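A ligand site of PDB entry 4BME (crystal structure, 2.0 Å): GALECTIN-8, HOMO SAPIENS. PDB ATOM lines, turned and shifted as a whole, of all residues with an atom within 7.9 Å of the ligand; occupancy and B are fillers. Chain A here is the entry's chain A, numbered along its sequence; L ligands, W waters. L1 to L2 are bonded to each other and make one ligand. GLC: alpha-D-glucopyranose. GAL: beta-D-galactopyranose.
The guanidinium group of Arg 66 lies within hydrogen-bond range of an oxygen (O3) of GLC L1, 2.6 Å away. OE2 of Glu 86 sits at hydrogen-bond distance from O6 of GAL L2, 2.7 Å away. An oxygen (O4) of GAL L2 lies within hydrogen-bond range of a ring nitrogen (NE2) of His 62, 2.9 Å away. ND2 of Asn 76 lies within hydrogen-bond range of O6 of GAL L2, at 3.0 Å. NH2 of Arg 42 lies within hydrogen-bond range of O3 of GAL L2 (3.1 Å). The side-chain amide oxygen (OD1) of Asn 64 sits at hydrogen-bond distance from an oxygen (O4) of GAL L2 (3.3 Å).
The side-chain amide oxygen (OD1) of Asn 64 is in hydrogen-bond range of the guanidinium group (NE) of Arg 66, 2.7 Å away. The backbone NH (N) of His 62 lies within hydrogen-bond range of the backbone carbonyl oxygen (O) of Asn 76, at 3.0 Å. The side-chain carboxylate of Asp 46 lies within hydrogen-bond range of a ring nitrogen (ND1) of His 62. The side-chain amide nitrogen (ND2) of Asn 76 is in hydrogen-bond range of the backbone carbonyl oxygen (O) of Gly 84, at 2.8 Å. The backbone carbonyl oxygen of Arg 85 lies close to the side-chain amide oxygen of Asn 76 (3.3 Å). The guanidinium group (NH1) of Arg 42 sits at hydrogen-bond distance from the side-chain amide oxygen (OD1) of Asn 64 (3.2 Å). The side-chain amide oxygen (OE1) of Gln 44 sits at hydrogen-bond distance from the guanidinium group (NH2) of Arg 42, at 2.9 Å. O of Phe 43 sits at hydrogen-bond distance from ND2 of Asn 64 (2.8 Å).
CG1 of Val 74 touches C6 of GAL L2 (3.9 Å). Trp 83 touches the ligand. Eight residues have an atom within 4 Å of the ligand: Arg 42, His 62, Asn 64, Arg 66, Val 74, Asn 76, Trp 83 and Glu 86.
Water W1 lies within hydrogen-bond range of O3 of GAL L2 (2.8 Å), NH2 of Arg 56 (3.0 Å) and NE2 of Gln 44 (3.5 Å).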
ATOM      1  N   ARG A  42       0.101  31.103  22.211  1.00  0.00           N
ATOM      2  CA  ARG A  42      -0.552  30.170  21.273  1.00  0.00           C
ATOM      3  C   ARG A  42      -1.725  30.859  20.576  1.00  0.00           C
ATOM      4  O   ARG A  42      -2.233  31.864  21.067  1.00  0.00           O
ATOM      5  CB  ARG A  42      -1.066  28.916  21.985  1.00  0.00           C
ATOM      6  CG  ARG A  42      -1.966  29.191  23.177  1.00  0.00           C
ATOM      7  CD  ARG A  42      -2.593  27.906  23.698  1.00  0.00           C
ATOM      8  NE  ARG A  42      -3.884  27.636  23.060  1.00  0.00           N
ATOM      9  CZ  ARG A  42      -4.570  26.500  23.188  1.00  0.00           C
ATOM     10  NH1 ARG A  42      -4.083  25.501  23.921  1.00  0.00           N
ATOM     11  NH2 ARG A  42      -5.738  26.357  22.578  1.00  0.00           N
ATOM     12  N   PHE A  43      -2.143  30.325  19.443  1.00  0.00           N
ATOM     13  CA  PHE A  43      -3.397  30.738  18.818  1.00  0.00           C
ATOM     14  C   PHE A  43      -4.011  29.557  18.078  1.00  0.00           C
ATOM     15  O   PHE A  43      -3.354  28.525  17.892  1.00  0.00           O
ATOM     16  CB  PHE A  43      -3.230  31.953  17.899  1.00  0.00           C
ATOM     17  CG  PHE A  43      -2.565  31.656  16.576  1.00  0.00           C
ATOM     18  CD1 PHE A  43      -3.310  31.242  15.480  1.00  0.00           C
ATOM     19  CD2 PHE A  43      -1.194  31.842  16.411  1.00  0.00           C
ATOM     20  CE1 PHE A  43      -2.696  30.968  14.243  1.00  0.00           C
ATOM     21  CE2 PHE A  43      -0.578  31.593  15.195  1.00  0.00           C
ATOM     22  CZ  PHE A  43      -1.344  31.156  14.101  1.00  0.00           C
ATOM     23  N   GLN A  44      -5.267  29.678  17.667  1.00  0.00           N
ATOM     24  CA  GLN A  44      -5.913  28.584  16.967  1.00  0.00           C
ATOM     25  C   GLN A  44      -6.823  29.024  15.832  1.00  0.00           C
ATOM     26  O   GLN A  44      -7.409  30.112  15.843  1.00  0.00           O
ATOM     27  CB  GLN A  44      -6.696  27.718  17.955  1.00  0.00           C
ATOM     28  CG  GLN A  44      -7.850  28.460  18.634  1.00  0.00           C
ATOM     29  CD  GLN A  44      -8.199  27.898  19.992  1.00  0.00           C
ATOM     30  OE1 GLN A  44      -7.428  28.035  20.943  1.00  0.00           O
ATOM     31  NE2 GLN A  44      -9.341  27.237  20.088  1.00  0.00           N
ATOM     32  N   ASP A  46     -10.088  27.321  14.152  1.00  0.00           N
ATOM     33  CA  ASP A  46     -11.038  26.252  14.405  1.00  0.00           C
ATOM     34  C   ASP A  46     -12.081  26.226  13.287  1.00  0.00           C
ATOM     35  O   ASP A  46     -12.739  27.232  13.016  1.00  0.00           O
ATOM     36  CB  ASP A  46     -11.746  26.482  15.762  1.00  0.00           C
ATOM     37  CG  ASP A  46     -10.829  26.264  16.954  1.00  0.00           C
ATOM     38  OD1 ASP A  46      -9.754  25.623  16.794  1.00  0.00           O
ATOM     39  OD2 ASP A  46     -11.196  26.700  18.054  1.00  0.00           O
ATOM     40  N   ARG A  56     -20.796  24.314  23.825  1.00  0.00           N
ATOM     41  CA  ARG A  56     -19.774  24.697  22.867  1.00  0.00           C
ATOM     42  C   ARG A  56     -19.923  23.898  21.566  1.00  0.00           C
ATOM     43  O   ARG A  56     -20.183  22.690  21.596  1.00  0.00           O
ATOM     44  CB  ARG A  56     -18.367  24.525  23.463  1.00  0.00           C
ATOM     45  CG  ARG A  56     -17.242  24.828  22.466  1.00  0.00           C
ATOM     46  CD  ARG A  56     -15.868  24.782  23.141  1.00  0.00           C
ATOM     47  NE  ARG A  56     -14.817  25.145  22.195  1.00  0.00           N
ATOM     48  CZ  ARG A  56     -13.517  25.080  22.469  1.00  0.00           C
ATOM     49  NH1 ARG A  56     -13.098  24.661  23.657  1.00  0.00           N
ATOM     50  NH2 ARG A  56     -12.627  25.440  21.552  1.00  0.00           N
ATOM     51  N   HIS A  62      -9.220  21.649  14.755  1.00  0.00           N
ATOM     52  CA  HIS A  62      -8.553  22.567  15.667  1.00  0.00           C
ATOM     53  C   HIS A  62      -7.076  22.573  15.263  1.00  0.00           C
ATOM     54  O   HIS A  62      -6.402  21.555  15.364  1.00  0.00           O
ATOM     55  CB  HIS A  62      -8.709  22.008  17.099  1.00  0.00           C
ATOM     56  CG  HIS A  62      -8.012  22.802  18.164  1.00  0.00           C
ATOM     57  ND1 HIS A  62      -8.127  24.168  18.295  1.00  0.00           N
ATOM     58  CD2 HIS A  62      -7.256  22.385  19.212  1.00  0.00           C
ATOM     59  CE1 HIS A  62      -7.438  24.572  19.347  1.00  0.00           C
ATOM     60  NE2 HIS A  62      -6.899  23.509  19.917  1.00  0.00           N
ATOM     61  N   PHE A  63      -6.603  23.719  14.788  1.00  0.00           N
ATOM     62  CA  PHE A  63      -5.232  23.868  14.305  1.00  0.00           C
ATOM     63  C   PHE A  63      -4.526  24.845  15.230  1.00  0.00           C
ATOM     64  O   PHE A  63      -4.735  26.049  15.110  1.00  0.00           O
ATOM     65  CB  PHE A  63      -5.273  24.404  12.866  1.00  0.00           C
ATOM     66  CG  PHE A  63      -3.928  24.690  12.270  1.00  0.00           C
ATOM     67  CD1 PHE A  63      -3.167  23.664  11.714  1.00  0.00           C
ATOM     68  CD2 PHE A  63      -3.426  25.994  12.225  1.00  0.00           C
ATOM     69  CE1 PHE A  63      -1.918  23.924  11.149  1.00  0.00           C
ATOM     70  CE2 PHE A  63      -2.188  26.272  11.663  1.00  0.00           C
ATOM     71  CZ  PHE A  63      -1.435  25.224  11.115  1.00  0.00           C
ATOM     72  N   ASN A  64      -3.723  24.337  16.156  1.00  0.00           N
ATOM     73  CA  ASN A  64      -3.305  25.120  17.337  1.00  0.00           C
ATOM     74  C   ASN A  64      -1.788  25.260  17.508  1.00  0.00           C
ATOM     75  O   ASN A  64      -1.166  24.487  18.240  1.00  0.00           O
ATOM     76  CB  ASN A  64      -3.993  24.557  18.595  1.00  0.00           C
ATOM     77  CG  ASN A  64      -3.507  25.201  19.901  1.00  0.00           C
ATOM     78  OD1 ASN A  64      -3.367  24.524  20.916  1.00  0.00           O
ATOM     79  ND2 ASN A  64      -3.269  26.506  19.884  1.00  0.00           N
ATOM     80  N   ARG A  66       1.473  26.436  19.132  1.00  0.00           N
ATOM     81  CA  ARG A  66       1.869  26.828  20.489  1.00  0.00           C
ATOM     82  C   ARG A  66       3.343  27.224  20.468  1.00  0.00           C
ATOM     83  O   ARG A  66       4.162  26.576  19.819  1.00  0.00           O
ATOM     84  CB  ARG A  66       1.629  25.673  21.461  1.00  0.00           C
ATOM     85  CG  ARG A  66       0.208  25.126  21.417  1.00  0.00           C
ATOM     86  CD  ARG A  66       0.011  24.012  22.416  1.00  0.00           C
ATOM     87  NE  ARG A  66      -1.372  23.542  22.419  1.00  0.00           N
ATOM     88  CZ  ARG A  66      -1.814  22.532  23.160  1.00  0.00           C
ATOM     89  NH1 ARG A  66      -0.977  21.877  23.962  1.00  0.00           N
ATOM     90  NH2 ARG A  66      -3.094  22.176  23.099  1.00  0.00           N
ATOM     91  N   CYS A  72       5.451  24.114  18.642  1.00  0.00           N
ATOM     92  CA  CYS A  72       4.708  23.015  18.018  1.00  0.00           C
ATOM     93  C   CYS A  72       3.326  23.424  17.488  1.00  0.00           C
ATOM     94  O   CYS A  72       2.854  24.535  17.721  1.00  0.00           O
ATOM     95  CB  CYS A  72       4.538  21.851  18.995  1.00  0.00           C
ATOM     96  SG  CYS A  72       3.376  22.151  20.356  1.00  0.00           S
ATOM     97  N   VAL A  74      -0.553  21.722  17.628  1.00  0.00           N
ATOM     98  CA  VAL A  74      -1.443  20.660  18.092  1.00  0.00           C
ATOM     99  C   VAL A  74      -2.708  20.664  17.243  1.00  0.00           C
ATOM    100  O   VAL A  74      -3.342  21.715  17.060  1.00  0.00           O
ATOM    101  CB  VAL A  74      -1.799  20.828  19.579  1.00  0.00           C
ATOM    102  CG1 VAL A  74      -2.752  19.738  20.019  1.00  0.00           C
ATOM    103  CG2 VAL A  74      -0.538  20.815  20.439  1.00  0.00           C
ATOM    104  N   CYS A  75      -3.059  19.504  16.677  1.00  0.00           N
ATOM    105  CA  CYS A  75      -4.353  19.377  16.012  1.00  0.00           C
ATOM    106  C   CYS A  75      -5.252  18.390  16.728  1.00  0.00           C
ATOM    107  O   CYS A  75      -4.784  17.382  17.262  1.00  0.00           O
ATOM    108  CB  CYS A  75      -4.204  19.004  14.538  1.00  0.00           C
ATOM    109  SG  CYS A  75      -3.225  20.174  13.594  1.00  0.00           S
ATOM    110  N   ASN A  76      -6.544  18.671  16.738  1.00  0.00           N
ATOM    111  CA  ASN A  76      -7.517  17.832  17.408  1.00  0.00           C
ATOM    112  C   ASN A  76      -8.962  18.138  16.934  1.00  0.00           C
ATOM    113  O   ASN A  76      -9.181  19.015  16.088  1.00  0.00           O
ATOM    114  CB  ASN A  76      -7.387  17.977  18.940  1.00  0.00           C
ATOM    115  CG  ASN A  76      -7.846  16.745  19.678  1.00  0.00           C
ATOM    116  OD1 ASN A  76      -8.480  15.859  19.099  1.00  0.00           O
ATOM    117  ND2 ASN A  76      -7.525  16.673  20.970  1.00  0.00           N
ATOM    118  N   THR A  77      -9.915  17.394  17.471  1.00  0.00           N
ATOM    119  CA  THR A  77     -11.321  17.548  17.122  1.00  0.00           C
ATOM    120  C   THR A  77     -12.090  17.548  18.436  1.00  0.00           C
ATOM    121  O   THR A  77     -11.801  16.742  19.342  1.00  0.00           O
ATOM    122  CB  THR A  77     -11.806  16.366  16.236  1.00  0.00           C
ATOM    123  OG1 THR A  77     -11.233  16.434  14.913  1.00  0.00           O
ATOM    124  CG2 THR A  77     -13.328  16.343  16.138  1.00  0.00           C
ATOM    125  N   LEU A  78     -13.031  18.477  18.560  1.00  0.00           N
ATOM    126  CA  LEU A  78     -13.903  18.548  19.731  1.00  0.00           C
ATOM    127  C   LEU A  78     -15.303  18.070  19.339  1.00  0.00           C
ATOM    128  O   LEU A  78     -15.939  18.641  18.452  1.00  0.00           O
ATOM    129  CB  LEU A  78     -13.976  19.982  20.263  1.00  0.00           C
ATOM    130  CG  LEU A  78     -14.818  20.201  21.522  1.00  0.00           C
ATOM    131  CD1 LEU A  78     -14.009  19.823  22.786  1.00  0.00           C
ATOM    132  CD2 LEU A  78     -15.358  21.640  21.594  1.00  0.00           C
ATOM    133  N   TRP A  83     -12.562  16.592  23.849  1.00  0.00           N
ATOM    134  CA  TRP A  83     -11.457  16.534  22.904  1.00  0.00           C
ATOM    135  C   TRP A  83     -11.032  15.103  22.598  1.00  0.00           C
ATOM    136  O   TRP A  83     -10.973  14.270  23.501  1.00  0.00           O
ATOM    137  CB  TRP A  83     -10.243  17.302  23.427  1.00  0.00           C
ATOM    138  CG  TRP A  83     -10.384  18.789  23.450  1.00  0.00           C
ATOM    139  CD1 TRP A  83     -10.491  19.584  24.555  1.00  0.00           C
ATOM    140  CD2 TRP A  83     -10.397  19.673  22.323  1.00  0.00           C
ATOM    141  NE1 TRP A  83     -10.569  20.905  24.189  1.00  0.00           N
ATOM    142  CE2 TRP A  83     -10.523  20.986  22.827  1.00  0.00           C
ATOM    143  CE3 TRP A  83     -10.325  19.476  20.936  1.00  0.00           C
ATOM    144  CZ2 TRP A  83     -10.577  22.103  21.982  1.00  0.00           C
ATOM    145  CZ3 TRP A  83     -10.378  20.582  20.110  1.00  0.00           C
ATOM    146  CH2 TRP A  83     -10.499  21.875  20.628  1.00  0.00           C
ATOM    147  N   GLY A  84     -10.727  14.818  21.337  1.00  0.00           N
ATOM    148  CA  GLY A  84     -10.259  13.499  20.928  1.00  0.00           C
ATOM    149  C   GLY A  84      -8.753  13.375  21.064  1.00  0.00           C
ATOM    150  O   GLY A  84      -8.143  14.082  21.865  1.00  0.00           O
ATOM    151  N   ARG A  85      -8.154  12.487  20.276  1.00  0.00           N
ATOM    152  CA  ARG A  85      -6.706  12.246  20.375  1.00  0.00           C
ATOM    153  C   ARG A  85      -5.870  13.319  19.679  1.00  0.00           C
ATOM    154  O   ARG A  85      -6.131  13.668  18.533  1.00  0.00           O
ATOM    155  CB  ARG A  85      -6.357  10.852  19.860  1.00  0.00           C
ATOM    156  CG  ARG A  85      -6.688   9.758  20.869  1.00  0.00           C
ATOM    157  CD  ARG A  85      -6.388   8.365  20.357  1.00  0.00           C
ATOM    158  NE  ARG A  85      -6.878   7.348  21.292  1.00  0.00           N
ATOM    159  CZ  ARG A  85      -6.737   6.034  21.118  1.00  0.00           C
ATOM    160  NH1 ARG A  85      -6.114   5.564  20.054  1.00  0.00           N
ATOM    161  NH2 ARG A  85      -7.217   5.201  22.033  1.00  0.00           N
ATOM    162  N   GLU A  86      -4.877  13.846  20.378  1.00  0.00           N
ATOM    163  CA  GLU A  86      -4.035  14.903  19.830  1.00  0.00           C
ATOM    164  C   GLU A  86      -3.090  14.387  18.750  1.00  0.00           C
ATOM    165  O   GLU A  86      -2.445  13.350  18.919  1.00  0.00           O
ATOM    166  CB  GLU A  86      -3.216  15.580  20.926  1.00  0.00           C
ATOM    167  CG  GLU A  86      -4.028  16.408  21.894  1.00  0.00           C
ATOM    168  CD  GLU A  86      -3.166  17.208  22.869  1.00  0.00           C
ATOM    169  OE1 GLU A  86      -2.050  16.748  23.190  1.00  0.00           O
ATOM    170  OE2 GLU A  86      -3.609  18.288  23.291  1.00  0.00           O
ATOM    171  N   GLU A  87      -3.040  15.103  17.631  1.00  0.00           N
ATOM    172  CA  GLU A  87      -2.007  14.884  16.628  1.00  0.00           C
ATOM    173  C   GLU A  87      -1.035  16.051  16.654  1.00  0.00           C
ATOM    174  O   GLU A  87      -1.387  17.168  16.290  1.00  0.00           O
ATOM    175  CB  GLU A  87      -2.625  14.741  15.238  1.00  0.00           C
ATOM    176  CG  GLU A  87      -3.276  13.405  15.051  1.00  0.00           C
ATOM    177  CD  GLU A  87      -3.988  13.283  13.722  1.00  0.00           C
ATOM    178  OE1 GLU A  87      -3.449  13.747  12.691  1.00  0.00           O
ATOM    179  OE2 GLU A  87      -5.104  12.718  13.707  1.00  0.00           O
ATOM    180  N   ILE A  88       0.194  15.785  17.072  1.00  0.00           N
ATOM    181  CA  ILE A  88       1.144  16.863  17.281  1.00  0.00           C
ATOM    182  C   ILE A  88       2.256  16.914  16.230  1.00  0.00           C
ATOM    183  O   ILE A  88       2.934  15.917  15.985  1.00  0.00           O
ATOM    184  CB  ILE A  88       1.785  16.789  18.684  1.00  0.00           C
ATOM    185  CG1 ILE A  88       0.716  16.708  19.773  1.00  0.00           C
ATOM    186  CG2 ILE A  88       2.706  17.979  18.917  1.00  0.00           C
ATOM    187  CD1 ILE A  88       1.288  16.351  21.152  1.00  0.00           C
HETATM  188  C1  GLC L   1      -2.889  17.836  27.916  1.00  0.00           C
HETATM  189  C2  GLC L   1      -2.386  18.385  26.587  1.00  0.00           C
HETATM  190  C3  GLC L   1      -2.977  19.780  26.356  1.00  0.00           C
HETATM  191  C4  GLC L   1      -4.501  19.752  26.522  1.00  0.00           C
HETATM  192  C5  GLC L   1      -4.902  19.036  27.826  1.00  0.00           C
HETATM  193  C6  GLC L   1      -6.411  18.874  27.993  1.00  0.00           C
HETATM  194  O1  GLC L   1      -2.530  18.746  28.936  1.00  0.00           O
HETATM  195  O2  GLC L   1      -0.971  18.421  26.569  1.00  0.00           O
HETATM  196  O3  GLC L   1      -2.628  20.244  25.069  1.00  0.00           O
HETATM  197  O4  GLC L   1      -5.030  21.066  26.479  1.00  0.00           O
HETATM  198  O5  GLC L   1      -4.294  17.755  27.874  1.00  0.00           O
HETATM  199  O6  GLC L   1      -6.978  20.126  28.298  1.00  0.00           O
HETATM  200  C1  GAL L   2      -6.026  21.315  25.500  1.00  0.00           C
HETATM  201  C2  GAL L   2      -6.416  22.783  25.475  1.00  0.00           C
HETATM  202  C3  GAL L   2      -7.414  23.045  24.357  1.00  0.00           C
HETATM  203  C4  GAL L   2      -6.937  22.421  23.051  1.00  0.00           C
HETATM  204  C5  GAL L   2      -6.570  20.963  23.262  1.00  0.00           C
HETATM  205  C6  GAL L   2      -6.072  20.318  21.984  1.00  0.00           C
HETATM  206  O2  GAL L   2      -7.021  23.121  26.719  1.00  0.00           O
HETATM  207  O3  GAL L   2      -7.585  24.440  24.205  1.00  0.00           O
HETATM  208  O4  GAL L   2      -5.808  23.098  22.546  1.00  0.00           O
HETATM  209  O5  GAL L   2      -5.547  20.895  24.235  1.00  0.00           O
HETATM  210  O6  GAL L   2      -5.949  18.929  22.190  1.00  0.00           O
HETATM  211  O   HOH W   1      -9.904  25.273  22.900  1.00  0.00           O
